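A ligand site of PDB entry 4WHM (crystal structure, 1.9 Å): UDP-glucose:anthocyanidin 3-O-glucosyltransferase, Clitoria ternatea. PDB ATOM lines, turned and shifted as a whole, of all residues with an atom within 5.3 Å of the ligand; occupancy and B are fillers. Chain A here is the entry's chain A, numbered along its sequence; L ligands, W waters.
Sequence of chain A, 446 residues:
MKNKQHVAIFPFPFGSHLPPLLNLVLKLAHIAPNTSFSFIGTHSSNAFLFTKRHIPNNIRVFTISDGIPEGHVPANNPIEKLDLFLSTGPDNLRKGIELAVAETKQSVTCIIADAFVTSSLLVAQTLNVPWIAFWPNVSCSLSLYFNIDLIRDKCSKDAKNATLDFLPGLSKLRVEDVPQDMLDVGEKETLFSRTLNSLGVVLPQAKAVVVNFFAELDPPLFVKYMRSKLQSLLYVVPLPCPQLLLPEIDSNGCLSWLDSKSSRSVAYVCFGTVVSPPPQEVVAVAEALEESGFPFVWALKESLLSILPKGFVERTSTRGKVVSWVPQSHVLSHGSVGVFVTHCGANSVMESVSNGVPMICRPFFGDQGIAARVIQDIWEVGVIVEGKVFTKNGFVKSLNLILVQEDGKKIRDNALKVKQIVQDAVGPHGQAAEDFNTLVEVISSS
The backbone NH (N) of Ser 348 is in hydrogen-bond range of an oxygen (O8) of the ligand, at 3.0 Å. The side-chain hydroxyl of Ser 348 sits at hydrogen-bond distance from an oxygen (O8) of the ligand, at 2.5 Å. The backbone NH (N) of Thr 273 lies within hydrogen-bond range of an oxygen (O11) of the ligand (2.7 Å). The side-chain hydroxyl (OG1) of Thr 273 lies within hydrogen-bond range of an oxygen (O11) of the ligand (2.6 Å). An oxygen (O10) of the ligand is in hydrogen-bond range of the side-chain hydroxyl of Ser 16. An oxygen (O3) of the ligand sits at hydrogen-bond distance from the side-chain carboxylate (OE1) of Glu 351, 2.6 Å away. The backbone NH (N) of Val 326 is in hydrogen-bond range of an oxygen (O2) of the ligand, at 3.2 Å. A nitrogen (N2) of the ligand lies within hydrogen-bond range of the backbone carbonyl oxygen (O) of Val 326. A ring nitrogen (NE2) of His 343 lies within hydrogen-bond range of an oxygen (O12) of the ligand, 2.9 Å away. An oxygen (O7) of the ligand sits at hydrogen-bond distance from the backbone NH (N) of Asn 347 (3.2 Å). The side-chain amide nitrogen (ND2) of Asn 347 lies within hydrogen-bond range of an oxygen (O7) of the ligand. The side-chain amide nitrogen (NE2) of Gln 328 lies close to an oxygen (O3) of the ligand, 3.3 Å away.
The side-chain hydroxyl (OG) of Ser 348 lies within hydrogen-bond range of the side-chain amide nitrogen (NE2) of Gln 328 (3.0 Å). The side-chain amide nitrogen (ND2) of Asn 347 is in hydrogen-bond range of the backbone carbonyl oxygen (O) of Ser 16. The side-chain amide nitrogen (NE2) of Gln 328 is in hydrogen-bond range of the side-chain carboxylate (OE1) of Glu 351 (3.0 Å). The backbone carbonyl oxygen (O) of His 343 sits close to the side-chain amide oxygen (OE1) of Gln 368, 3.4 Å away. The backbone carbonyl oxygen of Phe 271 sits close to a ring nitrogen (ND1) of His 343 (3.5 Å). The side-chain amide oxygen (OE1) of Gln 328 sits at hydrogen-bond distance from the side-chain hydroxyl (OH) of Tyr 268, 2.7 Å away. The side-chain sulfur (SG) of Cys 270 lies close to the backbone NH (N) of Gly 272 (3.5 Å). SG of Cys 270 sits at hydrogen-bond distance from O of Ala 299 (3.7 Å).
Cys 270 touches the ligand (SG to C3, 3.6 Å). Gly 272 touches the ligand (CA to O11, 3.7 Å). Val 274 touches the ligand. CB of Ala 299 touches O2 of the ligand, 3.7 Å away. Trp 325 touches the ligand. Gly 345 touches the ligand. Ala 346 touches the ligand. Hydrophobic or aromatic side chains that line the ligand: Val 274, Ala 299, Trp 325, Val 326 and His 343. 15 residues have an atom within 4 Å of the ligand: Ser 16, Cys 270, Gly 272, Thr 273, Val 274, Ala 299, Trp 325, Val 326, Gln 328, His 343, Gly 345, Ala 346, Asn 347, Ser 348 and Glu 351.
Water W6 bridges N of Ser 16 (2.8 Å) and O10 of the ligand (2.9 Å). Water W2 bridges O3 of the ligand and N of Ser 329. Water W1 lies within hydrogen-bond range of the backbone carbonyl oxygen (O) of Ser 324 (2.9 Å) and an oxygen (O2) of the ligand (2.9 Å). Water W8 lies within hydrogen-bond range of OE1 of Gln 328 (2.8 Å), OG of Ser 348 (3.0 Å), N of Gly 272 (3.5 Å) and SG of Cys 270 (3.5 Å).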
ATOM      1  N   SER A  16       4.033  26.837   3.550  1.00  0.00           N
ATOM      2  CA  SER A  16       3.886  25.720   2.623  1.00  0.00           C
ATOM      3  C   SER A  16       5.212  25.218   2.058  1.00  0.00           C
ATOM      4  O   SER A  16       5.234  24.241   1.311  1.00  0.00           O
ATOM      5  CB  SER A  16       2.960  26.107   1.483  1.00  0.00           C
ATOM      6  OG  SER A  16       3.592  27.072   0.673  1.00  0.00           O
ATOM      7  N   TYR A 268     -14.607  24.643  -6.079  1.00  0.00           N
ATOM      8  CA  TYR A 268     -13.865  24.778  -4.833  1.00  0.00           C
ATOM      9  C   TYR A 268     -12.997  26.018  -4.938  1.00  0.00           C
ATOM     10  O   TYR A 268     -12.286  26.207  -5.931  1.00  0.00           O
ATOM     11  CB  TYR A 268     -12.993  23.543  -4.569  1.00  0.00           C
ATOM     12  CG  TYR A 268     -12.001  23.786  -3.459  1.00  0.00           C
ATOM     13  CD1 TYR A 268     -12.434  24.155  -2.203  1.00  0.00           C
ATOM     14  CD2 TYR A 268     -10.628  23.663  -3.684  1.00  0.00           C
ATOM     15  CE1 TYR A 268     -11.542  24.386  -1.164  1.00  0.00           C
ATOM     16  CE2 TYR A 268      -9.718  23.888  -2.655  1.00  0.00           C
ATOM     17  CZ  TYR A 268     -10.185  24.258  -1.404  1.00  0.00           C
ATOM     18  OH  TYR A 268      -9.317  24.502  -0.358  1.00  0.00           O
ATOM     19  N   CYS A 270     -10.232  28.700  -3.062  1.00  0.00           N
ATOM     20  CA  CYS A 270      -9.313  28.994  -1.961  1.00  0.00           C
ATOM     21  C   CYS A 270      -8.109  29.779  -2.437  1.00  0.00           C
ATOM     22  O   CYS A 270      -7.521  29.447  -3.471  1.00  0.00           O
ATOM     23  CB  CYS A 270      -8.842  27.711  -1.281  1.00  0.00           C
ATOM     24  SG  CYS A 270      -7.914  28.033   0.236  1.00  0.00           S
ATOM     25  N   PHE A 271      -7.723  30.796  -1.682  1.00  0.00           N
ATOM     26  CA  PHE A 271      -6.583  31.607  -2.077  1.00  0.00           C
ATOM     27  C   PHE A 271      -5.316  31.311  -1.295  1.00  0.00           C
ATOM     28  O   PHE A 271      -4.361  32.078  -1.316  1.00  0.00           O
ATOM     29  CB  PHE A 271      -6.968  33.072  -2.040  1.00  0.00           C
ATOM     30  CG  PHE A 271      -8.168  33.368  -2.882  1.00  0.00           C
ATOM     31  CD1 PHE A 271      -8.249  32.827  -4.166  1.00  0.00           C
ATOM     32  CD2 PHE A 271      -9.214  34.119  -2.395  1.00  0.00           C
ATOM     33  CE1 PHE A 271      -9.346  33.073  -4.958  1.00  0.00           C
ATOM     34  CE2 PHE A 271     -10.324  34.372  -3.183  1.00  0.00           C
ATOM     35  CZ  PHE A 271     -10.387  33.845  -4.463  1.00  0.00           C
ATOM     36  N   GLY A 272      -5.313  30.155  -0.633  1.00  0.00           N
ATOM     37  CA  GLY A 272      -4.140  29.730   0.098  1.00  0.00           C
ATOM     38  C   GLY A 272      -4.049  30.344   1.484  1.00  0.00           C
ATOM     39  O   GLY A 272      -5.030  30.883   2.009  1.00  0.00           O
ATOM     40  N   THR A 273      -2.863  30.280   2.062  1.00  0.00           N
ATOM     41  CA  THR A 273      -2.694  30.613   3.462  1.00  0.00           C
ATOM     42  C   THR A 273      -1.969  31.937   3.674  1.00  0.00           C
ATOM     43  O   THR A 273      -1.794  32.373   4.813  1.00  0.00           O
ATOM     44  CB  THR A 273      -1.889  29.511   4.164  1.00  0.00           C
ATOM     45  OG1 THR A 273      -0.603  29.395   3.536  1.00  0.00           O
ATOM     46  CG2 THR A 273      -2.621  28.177   4.041  1.00  0.00           C
ATOM     47  N   VAL A 274      -1.560  32.581   2.583  1.00  0.00           N
ATOM     48  CA  VAL A 274      -0.764  33.818   2.686  1.00  0.00           C
ATOM     49  C   VAL A 274      -1.512  35.022   2.135  1.00  0.00           C
ATOM     50  O   VAL A 274      -1.583  36.061   2.787  1.00  0.00           O
ATOM     51  CB  VAL A 274       0.573  33.665   1.950  1.00  0.00           C
ATOM     52  CG1 VAL A 274       1.389  34.952   2.050  1.00  0.00           C
ATOM     53  CG2 VAL A 274       1.342  32.486   2.524  1.00  0.00           C
ATOM     54  N   VAL A 275      -2.050  34.874   0.930  1.00  0.00           N
ATOM     55  CA  VAL A 275      -2.781  35.939   0.239  1.00  0.00           C
ATOM     56  C   VAL A 275      -3.815  36.636   1.108  1.00  0.00           C
ATOM     57  O   VAL A 275      -4.711  36.004   1.662  1.00  0.00           O
ATOM     58  CB  VAL A 275      -3.535  35.382  -0.998  1.00  0.00           C
ATOM     59  CG1 VAL A 275      -4.488  36.427  -1.571  1.00  0.00           C
ATOM     60  CG2 VAL A 275      -2.538  34.943  -2.054  1.00  0.00           C
ATOM     61  N   ALA A 299     -13.060  27.887   1.030  1.00  0.00           N
ATOM     62  CA  ALA A 299     -12.217  27.923   2.209  1.00  0.00           C
ATOM     63  C   ALA A 299     -11.685  29.339   2.316  1.00  0.00           C
ATOM     64  O   ALA A 299     -10.945  29.811   1.453  1.00  0.00           O
ATOM     65  CB  ALA A 299     -11.084  26.920   2.082  1.00  0.00           C
ATOM     66  N   SER A 324     -13.571  27.851   7.278  1.00  0.00           N
ATOM     67  CA  SER A 324     -12.259  28.438   7.538  1.00  0.00           C
ATOM     68  C   SER A 324     -11.096  27.593   6.998  1.00  0.00           C
ATOM     69  O   SER A 324     -10.063  28.126   6.607  1.00  0.00           O
ATOM     70  CB  SER A 324     -12.065  28.681   9.035  1.00  0.00           C
ATOM     71  OG  SER A 324     -12.988  29.640   9.512  1.00  0.00           O
ATOM     72  N   TRP A 325     -11.278  26.277   6.990  1.00  0.00           N
ATOM     73  CA  TRP A 325     -10.212  25.348   6.612  1.00  0.00           C
ATOM     74  C   TRP A 325     -10.797  24.028   6.131  1.00  0.00           C
ATOM     75  O   TRP A 325     -11.788  23.540   6.680  1.00  0.00           O
ATOM     76  CB  TRP A 325      -9.298  25.109   7.826  1.00  0.00           C
ATOM     77  CG  TRP A 325      -8.131  24.220   7.523  1.00  0.00           C
ATOM     78  CD1 TRP A 325      -8.055  22.858   7.701  1.00  0.00           C
ATOM     79  CD2 TRP A 325      -6.862  24.621   6.981  1.00  0.00           C
ATOM     80  NE1 TRP A 325      -6.818  22.401   7.308  1.00  0.00           N
ATOM     81  CE2 TRP A 325      -6.069  23.454   6.870  1.00  0.00           C
ATOM     82  CE3 TRP A 325      -6.320  25.849   6.588  1.00  0.00           C
ATOM     83  CZ2 TRP A 325      -4.763  23.486   6.376  1.00  0.00           C
ATOM     84  CZ3 TRP A 325      -5.027  25.873   6.094  1.00  0.00           C
ATOM     85  CH2 TRP A 325      -4.264  24.705   5.996  1.00  0.00           C
ATOM     86  N   VAL A 326     -10.212  23.463   5.081  1.00  0.00           N
ATOM     87  CA  VAL A 326     -10.631  22.152   4.580  1.00  0.00           C
ATOM     88  C   VAL A 326      -9.399  21.276   4.397  1.00  0.00           C
ATOM     89  O   VAL A 326      -8.290  21.783   4.284  1.00  0.00           O
ATOM     90  CB  VAL A 326     -11.338  22.252   3.214  1.00  0.00           C
ATOM     91  CG1 VAL A 326     -12.568  23.132   3.303  1.00  0.00           C
ATOM     92  CG2 VAL A 326     -10.388  22.803   2.160  1.00  0.00           C
ATOM     93  N   PRO A 327      -9.595  19.945   4.401  1.00  0.00           N
ATOM     94  CA  PRO A 327      -8.509  19.057   3.977  1.00  0.00           C
ATOM     95  C   PRO A 327      -8.393  19.179   2.459  1.00  0.00           C
ATOM     96  O   PRO A 327      -9.023  18.409   1.734  1.00  0.00           O
ATOM     97  CB  PRO A 327      -9.021  17.671   4.381  1.00  0.00           C
ATOM     98  CG  PRO A 327     -10.515  17.800   4.393  1.00  0.00           C
ATOM     99  CD  PRO A 327     -10.791  19.208   4.834  1.00  0.00           C
ATOM    100  N   GLN A 328      -7.641  20.179   1.991  1.00  0.00           N
ATOM    101  CA  GLN A 328      -7.734  20.559   0.580  1.00  0.00           C
ATOM    102  C   GLN A 328      -7.354  19.437  -0.398  1.00  0.00           C
ATOM    103  O   GLN A 328      -8.026  19.259  -1.414  1.00  0.00           O
ATOM    104  CB  GLN A 328      -6.929  21.838   0.279  1.00  0.00           C
ATOM    105  CG  GLN A 328      -6.864  22.171  -1.222  1.00  0.00           C
ATOM    106  CD  GLN A 328      -6.243  23.512  -1.498  1.00  0.00           C
ATOM    107  OE1 GLN A 328      -6.706  24.537  -1.002  1.00  0.00           O
ATOM    108  NE2 GLN A 328      -5.188  23.521  -2.320  1.00  0.00           N
ATOM    109  N   SER A 329      -6.306  18.676  -0.104  1.00  0.00           N
ATOM    110  CA  SER A 329      -5.907  17.627  -1.041  1.00  0.00           C
ATOM    111  C   SER A 329      -7.004  16.553  -1.178  1.00  0.00           C
ATOM    112  O   SER A 329      -7.203  16.002  -2.257  1.00  0.00           O
ATOM    113  CB  SER A 329      -4.577  16.984  -0.629  1.00  0.00           C
ATOM    114  OG  SER A 329      -4.725  16.288   0.582  1.00  0.00           O
ATOM    115  N   HIS A 343      -5.205  30.738  -6.271  1.00  0.00           N
ATOM    116  CA  HIS A 343      -4.207  31.797  -6.413  1.00  0.00           C
ATOM    117  C   HIS A 343      -2.969  31.259  -7.137  1.00  0.00           C
ATOM    118  O   HIS A 343      -2.070  32.019  -7.450  1.00  0.00           O
ATOM    119  CB  HIS A 343      -3.816  32.362  -5.051  1.00  0.00           C
ATOM    120  CG  HIS A 343      -3.000  31.420  -4.207  1.00  0.00           C
ATOM    121  ND1 HIS A 343      -3.353  30.100  -4.005  1.00  0.00           N
ATOM    122  CD2 HIS A 343      -1.847  31.614  -3.520  1.00  0.00           C
ATOM    123  CE1 HIS A 343      -2.454  29.522  -3.221  1.00  0.00           C
ATOM    124  NE2 HIS A 343      -1.533  30.426  -2.910  1.00  0.00           N
ATOM    125  N   GLY A 345      -0.706  28.900  -5.957  1.00  0.00           N
ATOM    126  CA  GLY A 345       0.454  28.505  -5.179  1.00  0.00           C
ATOM    127  C   GLY A 345       0.890  27.138  -5.670  1.00  0.00           C
ATOM    128  O   GLY A 345       0.049  26.331  -6.074  1.00  0.00           O
ATOM    129  N   ALA A 346       2.192  26.856  -5.634  1.00  0.00           N
ATOM    130  CA  ALA A 346       2.714  25.624  -6.250  1.00  0.00           C
ATOM    131  C   ALA A 346       2.093  24.341  -5.689  1.00  0.00           C
ATOM    132  O   ALA A 346       1.824  23.394  -6.435  1.00  0.00           O
ATOM    133  CB  ALA A 346       4.241  25.578  -6.123  1.00  0.00           C
ATOM    134  N   ASN A 347       1.877  24.289  -4.385  1.00  0.00           N
ATOM    135  CA  ASN A 347       1.352  23.073  -3.792  1.00  0.00           C
ATOM    136  C   ASN A 347      -0.117  22.834  -4.162  1.00  0.00           C
ATOM    137  O   ASN A 347      -0.510  21.704  -4.450  1.00  0.00           O
ATOM    138  CB  ASN A 347       1.539  23.093  -2.286  1.00  0.00           C
ATOM    139  CG  ASN A 347       3.016  23.167  -1.914  1.00  0.00           C
ATOM    140  OD1 ASN A 347       3.765  22.206  -2.126  1.00  0.00           O
ATOM    141  ND2 ASN A 347       3.445  24.312  -1.394  1.00  0.00           N
ATOM    142  N   SER A 348      -0.899  23.906  -4.149  1.00  0.00           N
ATOM    143  CA  SER A 348      -2.294  23.833  -4.596  1.00  0.00           C
ATOM    144  C   SER A 348      -2.350  23.370  -6.041  1.00  0.00           C
ATOM    145  O   SER A 348      -3.171  22.512  -6.389  1.00  0.00           O
ATOM    146  CB  SER A 348      -2.982  25.203  -4.458  1.00  0.00           C
ATOM    147  OG  SER A 348      -3.152  25.542  -3.091  1.00  0.00           O
ATOM    148  N   VAL A 349      -1.478  23.916  -6.879  1.00  0.00           N
ATOM    149  CA  VAL A 349      -1.483  23.555  -8.292  1.00  0.00           C
ATOM    150  C   VAL A 349      -1.138  22.077  -8.453  1.00  0.00           C
ATOM    151  O   VAL A 349      -1.771  21.357  -9.231  1.00  0.00           O
ATOM    152  CB  VAL A 349      -0.544  24.444  -9.136  1.00  0.00           C
ATOM    153  CG1 VAL A 349      -0.416  23.899 -10.568  1.00  0.00           C
ATOM    154  CG2 VAL A 349      -1.069  25.877  -9.182  1.00  0.00           C
ATOM    155  N   GLU A 351      -1.660  19.675  -6.325  1.00  0.00           N
ATOM    156  CA  GLU A 351      -2.804  18.884  -5.861  1.00  0.00           C
ATOM    157  C   GLU A 351      -3.919  18.888  -6.893  1.00  0.00           C
ATOM    158  O   GLU A 351      -4.616  17.883  -7.082  1.00  0.00           O
ATOM    159  CB  GLU A 351      -3.327  19.434  -4.517  1.00  0.00           C
ATOM    160  CG  GLU A 351      -2.345  19.212  -3.333  1.00  0.00           C
ATOM    161  CD  GLU A 351      -2.473  20.259  -2.218  1.00  0.00           C
ATOM    162  OE1 GLU A 351      -3.456  21.031  -2.197  1.00  0.00           O
ATOM    163  OE2 GLU A 351      -1.561  20.311  -1.347  1.00  0.00           O
ATOM    164  N   PHE A 365       0.852  37.067  -6.177  1.00  0.00           N
ATOM    165  CA  PHE A 365       2.223  37.509  -5.946  1.00  0.00           C
ATOM    166  C   PHE A 365       3.251  36.451  -6.320  1.00  0.00           C
ATOM    167  O   PHE A 365       2.900  35.331  -6.692  1.00  0.00           O
ATOM    168  CB  PHE A 365       2.408  37.912  -4.481  1.00  0.00           C
ATOM    169  CG  PHE A 365       2.230  36.780  -3.489  1.00  0.00           C
ATOM    170  CD1 PHE A 365       3.278  35.923  -3.178  1.00  0.00           C
ATOM    171  CD2 PHE A 365       1.012  36.603  -2.858  1.00  0.00           C
ATOM    172  CE1 PHE A 365       3.115  34.887  -2.273  1.00  0.00           C
ATOM    173  CE2 PHE A 365       0.836  35.573  -1.949  1.00  0.00           C
ATOM    174  CZ  PHE A 365       1.886  34.711  -1.651  1.00  0.00           C
ATOM    175  N   GLN A 368       3.290  33.064  -8.797  1.00  0.00           N
ATOM    176  CA  GLN A 368       1.957  32.555  -9.109  1.00  0.00           C
ATOM    177  C   GLN A 368       1.552  32.883 -10.547  1.00  0.00           C
ATOM    178  O   GLN A 368       0.812  32.133 -11.195  1.00  0.00           O
ATOM    179  CB  GLN A 368       0.933  33.123  -8.121  1.00  0.00           C
ATOM    180  CG  GLN A 368       1.136  32.577  -6.693  1.00  0.00           C
ATOM    181  CD  GLN A 368       0.567  33.481  -5.616  1.00  0.00           C
ATOM    182  OE1 GLN A 368      -0.230  34.381  -5.888  1.00  0.00           O
ATOM    183  NE2 GLN A 368       0.974  33.234  -4.375  1.00  0.00           N
HETATM  184  N1  LIG L   1      -4.511  24.207   2.397  1.00  0.00           N
HETATM  185  C1  LIG L   1      -5.370  23.336   3.098  1.00  0.00           C
HETATM  186  N2  LIG L   1      -6.566  23.769   3.516  1.00  0.00           N
HETATM  187  C2  LIG L   1      -6.973  25.019   3.270  1.00  0.00           C
HETATM  188  C3  LIG L   1      -6.144  25.904   2.583  1.00  0.00           C
HETATM  189  C4  LIG L   1      -4.892  25.467   2.136  1.00  0.00           C
HETATM  190  O1  LIG L   1      -5.021  22.156   3.352  1.00  0.00           O
HETATM  191  O2  LIG L   1      -8.100  25.381   3.690  1.00  0.00           O
HETATM  192  C5  LIG L   1      -3.196  23.720   1.949  1.00  0.00           C
HETATM  193  C6  LIG L   1      -3.168  23.374   0.473  1.00  0.00           C
HETATM  194  O3  LIG L   1      -3.710  22.069   0.216  1.00  0.00           O
HETATM  195  C7  LIG L   1      -1.692  23.485   0.138  1.00  0.00           C
HETATM  196  C8  LIG L   1      -1.227  24.610   1.051  1.00  0.00           C
HETATM  197  O4  LIG L   1      -2.194  24.745   2.087  1.00  0.00           O
HETATM  198  O5  LIG L   1      -1.002  22.292   0.537  1.00  0.00           O
HETATM  199  C9  LIG L   1      -1.198  25.909   0.270  1.00  0.00           C
HETATM  200  O6  LIG L   1       0.095  26.104  -0.273  1.00  0.00           O
HETATM  201  P1  LIG L   1       0.267  26.831  -1.681  1.00  0.00           P
HETATM  202  O7  LIG L   1       1.690  26.588  -2.150  1.00  0.00           O
HETATM  203  O8  LIG L   1      -0.863  26.415  -2.595  1.00  0.00           O
HETATM  204  O9  LIG L   1      -0.018  28.395  -1.354  1.00  0.00           O
HETATM  205  P2  LIG L   1       0.412  29.320  -0.080  1.00  0.00           P
HETATM  206  O10 LIG L   1       1.821  28.914   0.311  1.00  0.00           O
HETATM  207  O11 LIG L   1      -0.643  29.082   0.981  1.00  0.00           O
HETATM  208  O12 LIG L   1       0.327  30.710  -0.667  1.00  0.00           O
HETATM  209  O   HOH W   1      -8.490  28.240   4.150  1.00  0.00           O
HETATM  210  O   HOH W   2      -3.949  19.533   1.626  1.00  0.00           O
HETATM  211  O   HOH W   3      -5.153  19.111   4.429  1.00  0.00           O
HETATM  212  O   HOH W   4      -0.609  21.313   3.100  1.00  0.00           O
HETATM  213  O   HOH W   5       3.017  30.835  -1.114  1.00  0.00           O
HETATM  214  O   HOH W   6       2.894  29.371   2.931  1.00  0.00           O
HETATM  215  O   HOH W   7      -1.769  32.252  -0.416  1.00  0.00           O
HETATM  216  O   HOH W   8      -4.947  26.735  -1.057  1.00  0.00           O
